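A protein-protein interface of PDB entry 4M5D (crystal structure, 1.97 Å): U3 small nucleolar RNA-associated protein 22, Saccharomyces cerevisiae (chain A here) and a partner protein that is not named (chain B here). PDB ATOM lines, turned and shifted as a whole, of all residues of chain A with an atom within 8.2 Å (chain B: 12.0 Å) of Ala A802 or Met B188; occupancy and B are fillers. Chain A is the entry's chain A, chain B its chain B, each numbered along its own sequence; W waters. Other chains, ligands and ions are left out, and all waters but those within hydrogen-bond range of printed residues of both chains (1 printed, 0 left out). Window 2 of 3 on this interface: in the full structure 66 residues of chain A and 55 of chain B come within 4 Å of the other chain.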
ATOM      1  N   LEU A 748      -9.659 -36.472  22.777  1.00  0.00           N
ATOM      2  CA  LEU A 748      -8.418 -36.244  23.527  1.00  0.00           C
ATOM      3  C   LEU A 748      -8.557 -37.025  24.817  1.00  0.00           C
ATOM      4  O   LEU A 748      -9.661 -37.175  25.324  1.00  0.00           O
ATOM      5  CB  LEU A 748      -8.208 -34.759  23.850  1.00  0.00           C
ATOM      6  CG  LEU A 748      -8.028 -33.761  22.709  1.00  0.00           C
ATOM      7  CD1 LEU A 748      -8.079 -32.323  23.237  1.00  0.00           C
ATOM      8  CD2 LEU A 748      -6.726 -34.015  21.936  1.00  0.00           C
ATOM      9  N   PHE A 786      -7.821 -31.839  29.569  1.00  0.00           N
ATOM     10  CA  PHE A 786      -7.419 -32.878  28.607  1.00  0.00           C
ATOM     11  C   PHE A 786      -5.929 -32.763  28.329  1.00  0.00           C
ATOM     12  O   PHE A 786      -5.304 -31.782  28.698  1.00  0.00           O
ATOM     13  CB  PHE A 786      -8.199 -32.745  27.301  1.00  0.00           C
ATOM     14  CG  PHE A 786      -9.676 -32.944  27.455  1.00  0.00           C
ATOM     15  CD1 PHE A 786     -10.232 -34.222  27.389  1.00  0.00           C
ATOM     16  CD2 PHE A 786     -10.522 -31.855  27.658  1.00  0.00           C
ATOM     17  CE1 PHE A 786     -11.606 -34.407  27.535  1.00  0.00           C
ATOM     18  CE2 PHE A 786     -11.898 -32.035  27.799  1.00  0.00           C
ATOM     19  CZ  PHE A 786     -12.437 -33.308  27.741  1.00  0.00           C
ATOM     20  N   LYS A 791      -4.996 -27.820  18.528  1.00  0.00           N
ATOM     21  CA  LYS A 791      -6.244 -27.619  17.789  1.00  0.00           C
ATOM     22  C   LYS A 791      -7.283 -26.730  18.486  1.00  0.00           C
ATOM     23  O   LYS A 791      -8.238 -26.290  17.844  1.00  0.00           O
ATOM     24  CB  LYS A 791      -6.870 -28.970  17.416  1.00  0.00           C
ATOM     25  CG  LYS A 791      -6.033 -29.783  16.446  1.00  0.00           C
ATOM     26  CD  LYS A 791      -6.538 -31.212  16.349  1.00  0.00           C
ATOM     27  CE  LYS A 791      -5.748 -32.005  15.328  1.00  0.00           C
ATOM     28  NZ  LYS A 791      -6.240 -33.412  15.257  1.00  0.00           N
ATOM     29  N   TRP A 792      -7.114 -26.471  19.784  1.00  0.00           N
ATOM     30  CA  TRP A 792      -7.996 -25.522  20.486  1.00  0.00           C
ATOM     31  C   TRP A 792      -8.016 -24.179  19.756  1.00  0.00           C
ATOM     32  O   TRP A 792      -6.954 -23.670  19.375  1.00  0.00           O
ATOM     33  CB  TRP A 792      -7.556 -25.298  21.931  1.00  0.00           C
ATOM     34  CG  TRP A 792      -7.643 -26.514  22.803  1.00  0.00           C
ATOM     35  CD1 TRP A 792      -6.603 -27.204  23.340  1.00  0.00           C
ATOM     36  CD2 TRP A 792      -8.839 -27.176  23.244  1.00  0.00           C
ATOM     37  NE1 TRP A 792      -7.064 -28.260  24.087  1.00  0.00           N
ATOM     38  CE2 TRP A 792      -8.435 -28.275  24.037  1.00  0.00           C
ATOM     39  CE3 TRP A 792     -10.211 -26.956  23.036  1.00  0.00           C
ATOM     40  CZ2 TRP A 792      -9.355 -29.152  24.641  1.00  0.00           C
ATOM     41  CZ3 TRP A 792     -11.133 -27.837  23.636  1.00  0.00           C
ATOM     42  CH2 TRP A 792     -10.695 -28.921  24.425  1.00  0.00           C
ATOM     43  N   PRO A 793      -9.223 -23.607  19.551  1.00  0.00           N
ATOM     44  CA  PRO A 793      -9.415 -22.277  18.963  1.00  0.00           C
ATOM     45  C   PRO A 793      -8.604 -21.175  19.662  1.00  0.00           C
ATOM     46  O   PRO A 793      -8.262 -21.315  20.840  1.00  0.00           O
ATOM     47  CB  PRO A 793     -10.910 -22.028  19.169  1.00  0.00           C
ATOM     48  CG  PRO A 793     -11.515 -23.384  19.123  1.00  0.00           C
ATOM     49  CD  PRO A 793     -10.513 -24.288  19.785  1.00  0.00           C
ATOM     50  N   GLU A 795      -9.520 -17.889  20.047  1.00  0.00           N
ATOM     51  CA  GLU A 795     -10.413 -16.790  20.378  1.00  0.00           C
ATOM     52  C   GLU A 795     -11.427 -17.389  21.367  1.00  0.00           C
ATOM     53  O   GLU A 795     -11.730 -18.576  21.282  1.00  0.00           O
ATOM     54  CB  GLU A 795     -11.061 -16.229  19.100  1.00  0.00           C
ATOM     55  CG  GLU A 795     -12.093 -15.138  19.324  1.00  0.00           C
ATOM     56  CD  GLU A 795     -13.475 -15.713  19.607  1.00  0.00           C
ATOM     57  OE1 GLU A 795     -13.731 -16.860  19.162  1.00  0.00           O
ATOM     58  OE2 GLU A 795     -14.277 -15.042  20.302  1.00  0.00           O
ATOM     59  N   ILE A 796     -11.921 -16.582  22.304  1.00  0.00           N
ATOM     60  CA  ILE A 796     -12.611 -17.118  23.491  1.00  0.00           C
ATOM     61  C   ILE A 796     -13.971 -17.772  23.216  1.00  0.00           C
ATOM     62  O   ILE A 796     -14.306 -18.768  23.850  1.00  0.00           O
ATOM     63  CB  ILE A 796     -12.720 -16.074  24.656  1.00  0.00           C
ATOM     64  CG1 ILE A 796     -13.080 -16.760  25.983  1.00  0.00           C
ATOM     65  CG2 ILE A 796     -13.717 -14.949  24.323  1.00  0.00           C
ATOM     66  CD1 ILE A 796     -11.986 -17.661  26.547  1.00  0.00           C
ATOM     67  N   THR A 797     -14.740 -17.222  22.276  1.00  0.00           N
ATOM     68  CA  THR A 797     -16.063 -17.768  21.935  1.00  0.00           C
ATOM     69  C   THR A 797     -15.925 -19.167  21.371  1.00  0.00           C
ATOM     70  O   THR A 797     -16.557 -20.108  21.855  1.00  0.00           O
ATOM     71  CB  THR A 797     -16.783 -16.888  20.901  1.00  0.00           C
ATOM     72  OG1 THR A 797     -16.870 -15.565  21.423  1.00  0.00           O
ATOM     73  CG2 THR A 797     -18.193 -17.397  20.644  1.00  0.00           C
ATOM     74  N   SER A 798     -15.095 -19.294  20.338  1.00  0.00           N
ATOM     75  CA  SER A 798     -14.827 -20.589  19.740  1.00  0.00           C
ATOM     76  C   SER A 798     -14.163 -21.538  20.729  1.00  0.00           C
ATOM     77  O   SER A 798     -14.465 -22.722  20.730  1.00  0.00           O
ATOM     78  CB  SER A 798     -13.964 -20.438  18.485  1.00  0.00           C
ATOM     79  OG  SER A 798     -14.516 -19.444  17.640  1.00  0.00           O
ATOM     80  N   LEU A 799     -13.263 -21.025  21.575  1.00  0.00           N
ATOM     81  CA  LEU A 799     -12.644 -21.882  22.590  1.00  0.00           C
ATOM     82  C   LEU A 799     -13.696 -22.492  23.513  1.00  0.00           C
ATOM     83  O   LEU A 799     -13.701 -23.704  23.735  1.00  0.00           O
ATOM     84  CB  LEU A 799     -11.564 -21.140  23.403  1.00  0.00           C
ATOM     85  CG  LEU A 799     -10.855 -21.987  24.463  1.00  0.00           C
ATOM     86  CD1 LEU A 799     -10.137 -23.193  23.821  1.00  0.00           C
ATOM     87  CD2 LEU A 799      -9.885 -21.155  25.319  1.00  0.00           C
ATOM     88  N   GLU A 800     -14.584 -21.660  24.053  1.00  0.00           N
ATOM     89  CA  GLU A 800     -15.608 -22.156  24.973  1.00  0.00           C
ATOM     90  C   GLU A 800     -16.554 -23.150  24.285  1.00  0.00           C
ATOM     91  O   GLU A 800     -16.970 -24.141  24.886  1.00  0.00           O
ATOM     92  CB  GLU A 800     -16.404 -21.005  25.615  1.00  0.00           C
ATOM     93  CG  GLU A 800     -15.617 -20.153  26.611  1.00  0.00           C
ATOM     94  CD  GLU A 800     -15.127 -20.924  27.842  1.00  0.00           C
ATOM     95  OE1 GLU A 800     -15.778 -21.916  28.266  1.00  0.00           O
ATOM     96  OE2 GLU A 800     -14.091 -20.513  28.413  1.00  0.00           O
ATOM     97  N   LYS A 801     -16.883 -22.895  23.022  1.00  0.00           N
ATOM     98  CA  LYS A 801     -17.769 -23.822  22.300  1.00  0.00           C
ATOM     99  C   LYS A 801     -17.082 -25.164  22.045  1.00  0.00           C
ATOM    100  O   LYS A 801     -17.710 -26.208  22.163  1.00  0.00           O
ATOM    101  CB  LYS A 801     -18.295 -23.202  21.010  1.00  0.00           C
ATOM    102  CG  LYS A 801     -19.318 -22.106  21.255  1.00  0.00           C
ATOM    103  CD  LYS A 801     -19.834 -21.580  19.923  1.00  0.00           C
ATOM    104  CE  LYS A 801     -20.504 -20.235  20.072  1.00  0.00           C
ATOM    105  NZ  LYS A 801     -21.754 -20.370  20.843  1.00  0.00           N
ATOM    106  N   ALA A 802     -15.785 -25.133  21.740  1.00  0.00           N
ATOM    107  CA  ALA A 802     -15.000 -26.363  21.593  1.00  0.00           C
ATOM    108  C   ALA A 802     -14.948 -27.187  22.884  1.00  0.00           C
ATOM    109  O   ALA A 802     -15.022 -28.432  22.849  1.00  0.00           O
ATOM    110  CB  ALA A 802     -13.597 -26.041  21.105  1.00  0.00           C
ATOM    111  N   LYS A 803     -14.798 -26.498  24.019  1.00  0.00           N
ATOM    112  CA  LYS A 803     -14.830 -27.147  25.340  1.00  0.00           C
ATOM    113  C   LYS A 803     -16.200 -27.812  25.548  1.00  0.00           C
ATOM    114  O   LYS A 803     -16.309 -28.939  26.031  1.00  0.00           O
ATOM    115  CB  LYS A 803     -14.644 -26.102  26.458  1.00  0.00           C
ATOM    116  CG  LYS A 803     -13.263 -25.446  26.625  1.00  0.00           C
ATOM    117  CD  LYS A 803     -13.417 -24.358  27.733  1.00  0.00           C
ATOM    118  CE  LYS A 803     -12.151 -23.648  28.126  1.00  0.00           C
ATOM    119  NZ  LYS A 803     -12.451 -22.710  29.280  1.00  0.00           N
ATOM    120  N   THR A 804     -17.252 -27.072  25.226  1.00  0.00           N
ATOM    121  CA  THR A 804     -18.619 -27.559  25.391  1.00  0.00           C
ATOM    122  C   THR A 804     -18.849 -28.805  24.538  1.00  0.00           C
ATOM    123  O   THR A 804     -19.540 -29.732  24.957  1.00  0.00           O
ATOM    124  CB  THR A 804     -19.619 -26.456  25.047  1.00  0.00           C
ATOM    125  OG1 THR A 804     -19.409 -25.367  25.945  1.00  0.00           O
ATOM    126  CG2 THR A 804     -21.063 -26.943  25.217  1.00  0.00           C
ATOM    127  N   ALA A 805     -18.228 -28.830  23.361  1.00  0.00           N
ATOM    128  CA  ALA A 805     -18.301 -29.996  22.478  1.00  0.00           C
ATOM    129  C   ALA A 805     -17.748 -31.252  23.156  1.00  0.00           C
ATOM    130  O   ALA A 805     -18.307 -32.339  22.986  1.00  0.00           O
ATOM    131  CB  ALA A 805     -17.589 -29.724  21.151  1.00  0.00           C
ATOM    132  N   PHE A 806     -16.673 -31.106  23.944  1.00  0.00           N
ATOM    133  CA  PHE A 806     -16.133 -32.240  24.692  1.00  0.00           C
ATOM    134  C   PHE A 806     -17.053 -32.663  25.839  1.00  0.00           C
ATOM    135  O   PHE A 806     -17.240 -33.861  26.097  1.00  0.00           O
ATOM    136  CB  PHE A 806     -14.711 -31.948  25.208  1.00  0.00           C
ATOM    137  CG  PHE A 806     -13.640 -32.210  24.189  1.00  0.00           C
ATOM    138  CD1 PHE A 806     -13.309 -31.242  23.241  1.00  0.00           C
ATOM    139  CD2 PHE A 806     -12.970 -33.424  24.168  1.00  0.00           C
ATOM    140  CE1 PHE A 806     -12.320 -31.481  22.284  1.00  0.00           C
ATOM    141  CE2 PHE A 806     -11.976 -33.680  23.206  1.00  0.00           C
ATOM    142  CZ  PHE A 806     -11.654 -32.706  22.271  1.00  0.00           C
ATOM    143  N   LEU A 807     -17.633 -31.687  26.525  1.00  0.00           N
ATOM    144  CA  LEU A 807     -18.593 -31.996  27.583  1.00  0.00           C
ATOM    145  C   LEU A 807     -19.813 -32.740  27.037  1.00  0.00           C
ATOM    146  O   LEU A 807     -20.351 -33.629  27.695  1.00  0.00           O
ATOM    147  CB  LEU A 807     -19.032 -30.730  28.317  1.00  0.00           C
ATOM    148  CG  LEU A 807     -17.965 -30.011  29.158  1.00  0.00           C
ATOM    149  CD1 LEU A 807     -18.534 -28.710  29.720  1.00  0.00           C
ATOM    150  CD2 LEU A 807     -17.478 -30.924  30.293  1.00  0.00           C
ATOM    151  N   LEU A 808     -20.260 -32.348  25.850  1.00  0.00           N
ATOM    152  CA  LEU A 808     -21.358 -33.056  25.170  1.00  0.00           C
ATOM    153  C   LEU A 808     -21.011 -34.538  24.921  1.00  0.00           C
ATOM    154  O   LEU A 808     -21.840 -35.423  25.146  1.00  0.00           O
ATOM    155  CB  LEU A 808     -21.736 -32.351  23.864  1.00  0.00           C
ATOM    156  CG  LEU A 808     -22.601 -31.094  24.015  1.00  0.00           C
ATOM    157  CD1 LEU A 808     -22.660 -30.328  22.704  1.00  0.00           C
ATOM    158  CD2 LEU A 808     -24.012 -31.473  24.478  1.00  0.00           C
ATOM    159  N   LYS A 809     -19.774 -34.799  24.508  1.00  0.00           N
ATOM    160  CA  LYS A 809     -19.312 -36.176  24.293  1.00  0.00           C
ATOM    161  C   LYS A 809     -19.271 -36.967  25.602  1.00  0.00           C
ATOM    162  O   LYS A 809     -19.656 -38.139  25.639  1.00  0.00           O
ATOM    163  CB  LYS A 809     -17.953 -36.201  23.588  1.00  0.00           C
ATOM    164  CG  LYS A 809     -18.005 -35.662  22.169  1.00  0.00           C
ATOM    165  CD  LYS A 809     -16.781 -36.068  21.359  1.00  0.00           C
ATOM    166  CE  LYS A 809     -16.914 -35.640  19.892  1.00  0.00           C
ATOM    167  NZ  LYS A 809     -18.027 -36.340  19.170  1.00  0.00           N
ATOM    168  N   GLU A 836     -20.054 -17.582  27.044  1.00  0.00           N
ATOM    169  CA  GLU A 836     -20.218 -18.921  26.466  1.00  0.00           C
ATOM    170  C   GLU A 836     -19.734 -20.080  27.340  1.00  0.00           C
ATOM    171  O   GLU A 836     -19.646 -21.211  26.863  1.00  0.00           O
ATOM    172  CB  GLU A 836     -19.492 -19.002  25.115  1.00  0.00           C
ATOM    173  CG  GLU A 836     -19.999 -18.032  24.057  1.00  0.00           C
ATOM    174  CD  GLU A 836     -21.453 -18.259  23.719  1.00  0.00           C
ATOM    175  OE1 GLU A 836     -21.903 -19.425  23.700  1.00  0.00           O
ATOM    176  OE2 GLU A 836     -22.157 -17.263  23.495  1.00  0.00           O
ATOM    177  N   VAL A 854     -14.226 -27.169  31.667  1.00  0.00           N
ATOM    178  CA  VAL A 854     -12.992 -27.550  30.982  1.00  0.00           C
ATOM    179  C   VAL A 854     -11.984 -26.418  31.064  1.00  0.00           C
ATOM    180  O   VAL A 854     -12.331 -25.246  30.913  1.00  0.00           O
ATOM    181  CB  VAL A 854     -13.227 -27.972  29.519  1.00  0.00           C
ATOM    182  CG1 VAL A 854     -11.895 -28.352  28.843  1.00  0.00           C
ATOM    183  CG2 VAL A 854     -14.205 -29.157  29.467  1.00  0.00           C
ATOM    184  N   THR A 856      -8.210 -25.348  29.425  1.00  0.00           N
ATOM    185  CA  THR A 856      -7.177 -25.643  28.432  1.00  0.00           C
ATOM    186  C   THR A 856      -5.952 -24.765  28.642  1.00  0.00           C
ATOM    187  O   THR A 856      -6.002 -23.767  29.361  1.00  0.00           O
ATOM    188  CB  THR A 856      -7.659 -25.462  26.966  1.00  0.00           C
ATOM    189  OG1 THR A 856      -7.757 -24.064  26.655  1.00  0.00           O
ATOM    190  CG2 THR A 856      -9.018 -26.160  26.735  1.00  0.00           C
ATOM    191  N   SER B 101     -14.840 -11.311  23.128  1.00  0.00           N
ATOM    192  CA  SER B 101     -14.558 -11.988  21.863  1.00  0.00           C
ATOM    193  C   SER B 101     -13.615 -11.195  20.955  1.00  0.00           C
ATOM    194  O   SER B 101     -12.607 -11.725  20.471  1.00  0.00           O
ATOM    195  CB  SER B 101     -15.863 -12.282  21.118  1.00  0.00           C
ATOM    196  OG  SER B 101     -15.596 -12.834  19.844  1.00  0.00           O
ATOM    197  N   TYR B 179     -31.057 -27.215  21.493  1.00  0.00           N
ATOM    198  CA  TYR B 179     -30.543 -25.920  21.059  1.00  0.00           C
ATOM    199  C   TYR B 179     -29.023 -25.873  21.216  1.00  0.00           C
ATOM    200  O   TYR B 179     -28.306 -25.471  20.294  1.00  0.00           O
ATOM    201  CB  TYR B 179     -31.192 -24.785  21.851  1.00  0.00           C
ATOM    202  CG  TYR B 179     -32.503 -24.297  21.269  1.00  0.00           C
ATOM    203  CD1 TYR B 179     -33.720 -24.888  21.635  1.00  0.00           C
ATOM    204  CD2 TYR B 179     -32.530 -23.242  20.354  1.00  0.00           C
ATOM    205  CE1 TYR B 179     -34.934 -24.444  21.102  1.00  0.00           C
ATOM    206  CE2 TYR B 179     -33.742 -22.784  19.812  1.00  0.00           C
ATOM    207  CZ  TYR B 179     -34.935 -23.390  20.193  1.00  0.00           C
ATOM    208  OH  TYR B 179     -36.124 -22.943  19.664  1.00  0.00           O
ATOM    209  N   LEU B 180     -28.541 -26.304  22.383  1.00  0.00           N
ATOM    210  CA  LEU B 180     -27.106 -26.336  22.663  1.00  0.00           C
ATOM    211  C   LEU B 180     -26.360 -27.214  21.659  1.00  0.00           C
ATOM    212  O   LEU B 180     -25.410 -26.760  21.022  1.00  0.00           O
ATOM    213  CB  LEU B 180     -26.827 -26.797  24.098  1.00  0.00           C
ATOM    214  CG  LEU B 180     -25.351 -26.810  24.520  1.00  0.00           C
ATOM    215  CD1 LEU B 180     -24.744 -25.398  24.498  1.00  0.00           C
ATOM    216  CD2 LEU B 180     -25.208 -27.447  25.890  1.00  0.00           C
ATOM    217  N   LYS B 181     -26.803 -28.463  21.518  1.00  0.00           N
ATOM    218  CA  LYS B 181     -26.200 -29.387  20.554  1.00  0.00           C
ATOM    219  C   LYS B 181     -26.098 -28.745  19.177  1.00  0.00           C
ATOM    220  O   LYS B 181     -25.027 -28.724  18.579  1.00  0.00           O
ATOM    221  CB  LYS B 181     -26.980 -30.701  20.475  1.00  0.00           C
ATOM    222  CG  LYS B 181     -26.620 -31.696  21.555  1.00  0.00           C
ATOM    223  CD  LYS B 181     -27.575 -32.875  21.567  1.00  0.00           C
ATOM    224  CE  LYS B 181     -27.372 -33.710  22.822  1.00  0.00           C
ATOM    225  NZ  LYS B 181     -28.365 -34.815  22.942  1.00  0.00           N
ATOM    226  N   GLU B 182     -27.208 -28.191  18.697  1.00  0.00           N
ATOM    227  CA  GLU B 182     -27.230 -27.537  17.392  1.00  0.00           C
ATOM    228  C   GLU B 182     -26.224 -26.386  17.311  1.00  0.00           C
ATOM    229  O   GLU B 182     -25.400 -26.345  16.399  1.00  0.00           O
ATOM    230  CB  GLU B 182     -28.647 -27.063  17.038  1.00  0.00           C
ATOM    231  CG  GLU B 182     -28.858 -26.800  15.552  1.00  0.00           C
ATOM    232  CD  GLU B 182     -28.514 -28.001  14.678  1.00  0.00           C
ATOM    233  OE1 GLU B 182     -29.353 -28.924  14.560  1.00  0.00           O
ATOM    234  OE2 GLU B 182     -27.405 -28.019  14.097  1.00  0.00           O
ATOM    235  N   ASP B 183     -26.294 -25.472  18.277  1.00  0.00           N
ATOM    236  CA  ASP B 183     -25.371 -24.344  18.374  1.00  0.00           C
ATOM    237  C   ASP B 183     -23.905 -24.789  18.286  1.00  0.00           C
ATOM    238  O   ASP B 183     -23.140 -24.273  17.464  1.00  0.00           O
ATOM    239  CB  ASP B 183     -25.630 -23.564  19.674  1.00  0.00           C
ATOM    240  CG  ASP B 183     -24.620 -22.449  19.910  1.00  0.00           C
ATOM    241  OD1 ASP B 183     -24.216 -21.782  18.934  1.00  0.00           O
ATOM    242  OD2 ASP B 183     -24.237 -22.234  21.083  1.00  0.00           O
ATOM    243  N   ILE B 184     -23.525 -25.758  19.119  1.00  0.00           N
ATOM    244  CA  ILE B 184     -22.146 -26.238  19.162  1.00  0.00           C
ATOM    245  C   ILE B 184     -21.741 -26.958  17.867  1.00  0.00           C
ATOM    246  O   ILE B 184     -20.692 -26.657  17.293  1.00  0.00           O
ATOM    247  CB  ILE B 184     -21.881 -27.140  20.407  1.00  0.00           C
ATOM    248  CG1 ILE B 184     -22.247 -26.412  21.713  1.00  0.00           C
ATOM    249  CG2 ILE B 184     -20.441 -27.619  20.434  1.00  0.00           C
ATOM    250  CD1 ILE B 184     -21.563 -25.050  21.926  1.00  0.00           C
ATOM    251  N   HIS B 185     -22.580 -27.897  17.419  1.00  0.00           N
ATOM    252  CA  HIS B 185     -22.312 -28.704  16.220  1.00  0.00           C
ATOM    253  C   HIS B 185     -22.073 -27.829  14.982  1.00  0.00           C
ATOM    254  O   HIS B 185     -21.105 -28.048  14.250  1.00  0.00           O
ATOM    255  CB  HIS B 185     -23.449 -29.714  15.966  1.00  0.00           C
ATOM    256  CG  HIS B 185     -23.483 -30.866  16.931  1.00  0.00           C
ATOM    257  ND1 HIS B 185     -23.877 -32.135  16.559  1.00  0.00           N
ATOM    258  CD2 HIS B 185     -23.172 -30.945  18.250  1.00  0.00           C
ATOM    259  CE1 HIS B 185     -23.814 -32.941  17.604  1.00  0.00           C
ATOM    260  NE2 HIS B 185     -23.389 -32.244  18.643  1.00  0.00           N
ATOM    261  N   THR B 186     -22.943 -26.838  14.771  1.00  0.00           N
ATOM    262  CA  THR B 186     -22.810 -25.891  13.651  1.00  0.00           C
ATOM    263  C   THR B 186     -21.568 -25.008  13.755  1.00  0.00           C
ATOM    264  O   THR B 186     -20.801 -24.908  12.795  1.00  0.00           O
ATOM    265  CB  THR B 186     -24.059 -24.975  13.462  1.00  0.00           C
ATOM    266  OG1 THR B 186     -24.263 -24.172  14.630  1.00  0.00           O
ATOM    267  CG2 THR B 186     -25.310 -25.790  13.176  1.00  0.00           C
ATOM    268  N   HIS B 187     -21.369 -24.373  14.913  1.00  0.00           N
ATOM    269  CA  HIS B 187     -20.215 -23.488  15.116  1.00  0.00           C
ATOM    270  C   HIS B 187     -18.878 -24.199  14.914  1.00  0.00           C
ATOM    271  O   HIS B 187     -17.928 -23.603  14.413  1.00  0.00           O
ATOM    272  CB  HIS B 187     -20.271 -22.799  16.484  1.00  0.00           C
ATOM    273  CG  HIS B 187     -20.950 -21.461  16.460  1.00  0.00           C
ATOM    274  ND1 HIS B 187     -20.257 -20.271  16.549  1.00  0.00           N
ATOM    275  CD2 HIS B 187     -22.259 -21.125  16.353  1.00  0.00           C
ATOM    276  CE1 HIS B 187     -21.109 -19.261  16.505  1.00  0.00           C
ATOM    277  NE2 HIS B 187     -22.329 -19.752  16.384  1.00  0.00           N
ATOM    278  N   MET B 188     -18.824 -25.478  15.287  1.00  0.00           N
ATOM    279  CA  MET B 188     -17.602 -26.282  15.178  1.00  0.00           C
ATOM    280  C   MET B 188     -17.319 -26.818  13.768  1.00  0.00           C
ATOM    281  O   MET B 188     -16.206 -27.277  13.489  1.00  0.00           O
ATOM    282  CB  MET B 188     -17.609 -27.427  16.199  1.00  0.00           C
ATOM    283  CG  MET B 188     -17.411 -26.988  17.654  1.00  0.00           C
ATOM    284  SD  MET B 188     -15.795 -26.235  17.993  1.00  0.00           S
ATOM    285  CE  MET B 188     -16.138 -24.479  17.844  1.00  0.00           C
ATOM    286  N   ALA B 189     -18.319 -26.757  12.890  1.00  0.00           N
ATOM    287  CA  ALA B 189     -18.168 -27.226  11.509  1.00  0.00           C
ATOM    288  C   ALA B 189     -17.298 -26.283  10.676  1.00  0.00           C
ATOM    289  O   ALA B 189     -17.416 -25.060  10.773  1.00  0.00           O
ATOM    290  CB  ALA B 189     -19.534 -27.418  10.859  1.00  0.00           C
HETATM  291  O   HOH W   1     -17.548 -20.423  17.008  1.00  0.00           O
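Water W1 bridges ND1 of His B187 (2.8 Å) and OG of Ser A798 (3.2 Å).
The side-chain hydroxyl (OG1) of Thr B186 is in hydrogen-bond range of the backbone carbonyl oxygen (O) of Asp B183 (3.1 Å).
The side-chain amino group of Lys A801 lies within salt-bridge range of the side-chain carboxylate of Glu A836 (3.0 Å).
OE2 of Glu A795 lies within hydrogen-bond range of OG1 of Thr A797 (2.9 Å).
OE1 of Glu A795 lies within hydrogen-bond range of N of Ser A798 (3.0 Å).
OG1 of Thr A804 is in hydrogen-bond range of O of Glu A800, 2.9 Å away.
Of chain B, only Met B188 comes within 4 Å of Ala A802.
Of the printed residues of chain A, Met B188 touches Ser A798 and Ala A802.
No residue of chain B comes within 4 Å of Trp A792.
No residue of chain B comes within 4 Å of Pro A793.
Ser A798 touches just one residue of chain B: Met B188.
Printed residues of chain B within 4 Å of Lys A801: Asp B183, Ile B184 and His B187.
Printed residues of chain B within 4 Å of Thr A804: Ile B184.
Ala A805 touches one residue of chain B.
No residue of chain B comes within 4 Å of Phe A806.
No residue of chain A comes within 4 Å of Ala B189.
Of the printed residues of chain A, Ser B101 touches Glu A795 (2.6 Å), Ile A796 (3.9 Å) and Thr A797 (3.4 Å).
Of the printed residues of chain A, His B187 touches Lys A801 (3.5 Å).
Leu B180 touches none of the printed residues of chain A.
The nearest residue of chain B that does not touch Ala A802 is Ile B184 (5.4 Å).
OG of Ser B101 is in hydrogen-bond range of OE2 of Glu A795 (2.6 Å).
OG of Ser B101 is in hydrogen-bond range of OG1 of Thr A797, 3.4 Å away.
The side-chain amino group (NZ) of Lys A801 is in salt-bridge range of the side-chain carboxylate (OD2) of Asp B183, at 3.1 Å.
Of the 23 printed residues of chain A, 9 touch a printed residue of chain B.
Among the printed residues, 11 pairs touch across the chains.
Among the printed residues, Asp or Glu carboxylates within 4 Å of a Lys or Arg side-chain nitrogen of the other chain: Lys A801 with Asp B183 (3.1 Å).
Ile A796 touches Ser B101 (CG2 to CA, 3.9 Å).
Met B188 touches Ser A798 (CE to O, 3.8 Å).
Ile B184 touches Lys A801 (CG2 to O, 3.5 Å).
Lys A801 touches His B187.
Ala A802 touches Met B188.
Thr A804 touches Ile B184 (CG2 to CG1, 3.7 Å).
Ile B184 touches Ala A805.
Leu A808 touches Lys B181.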
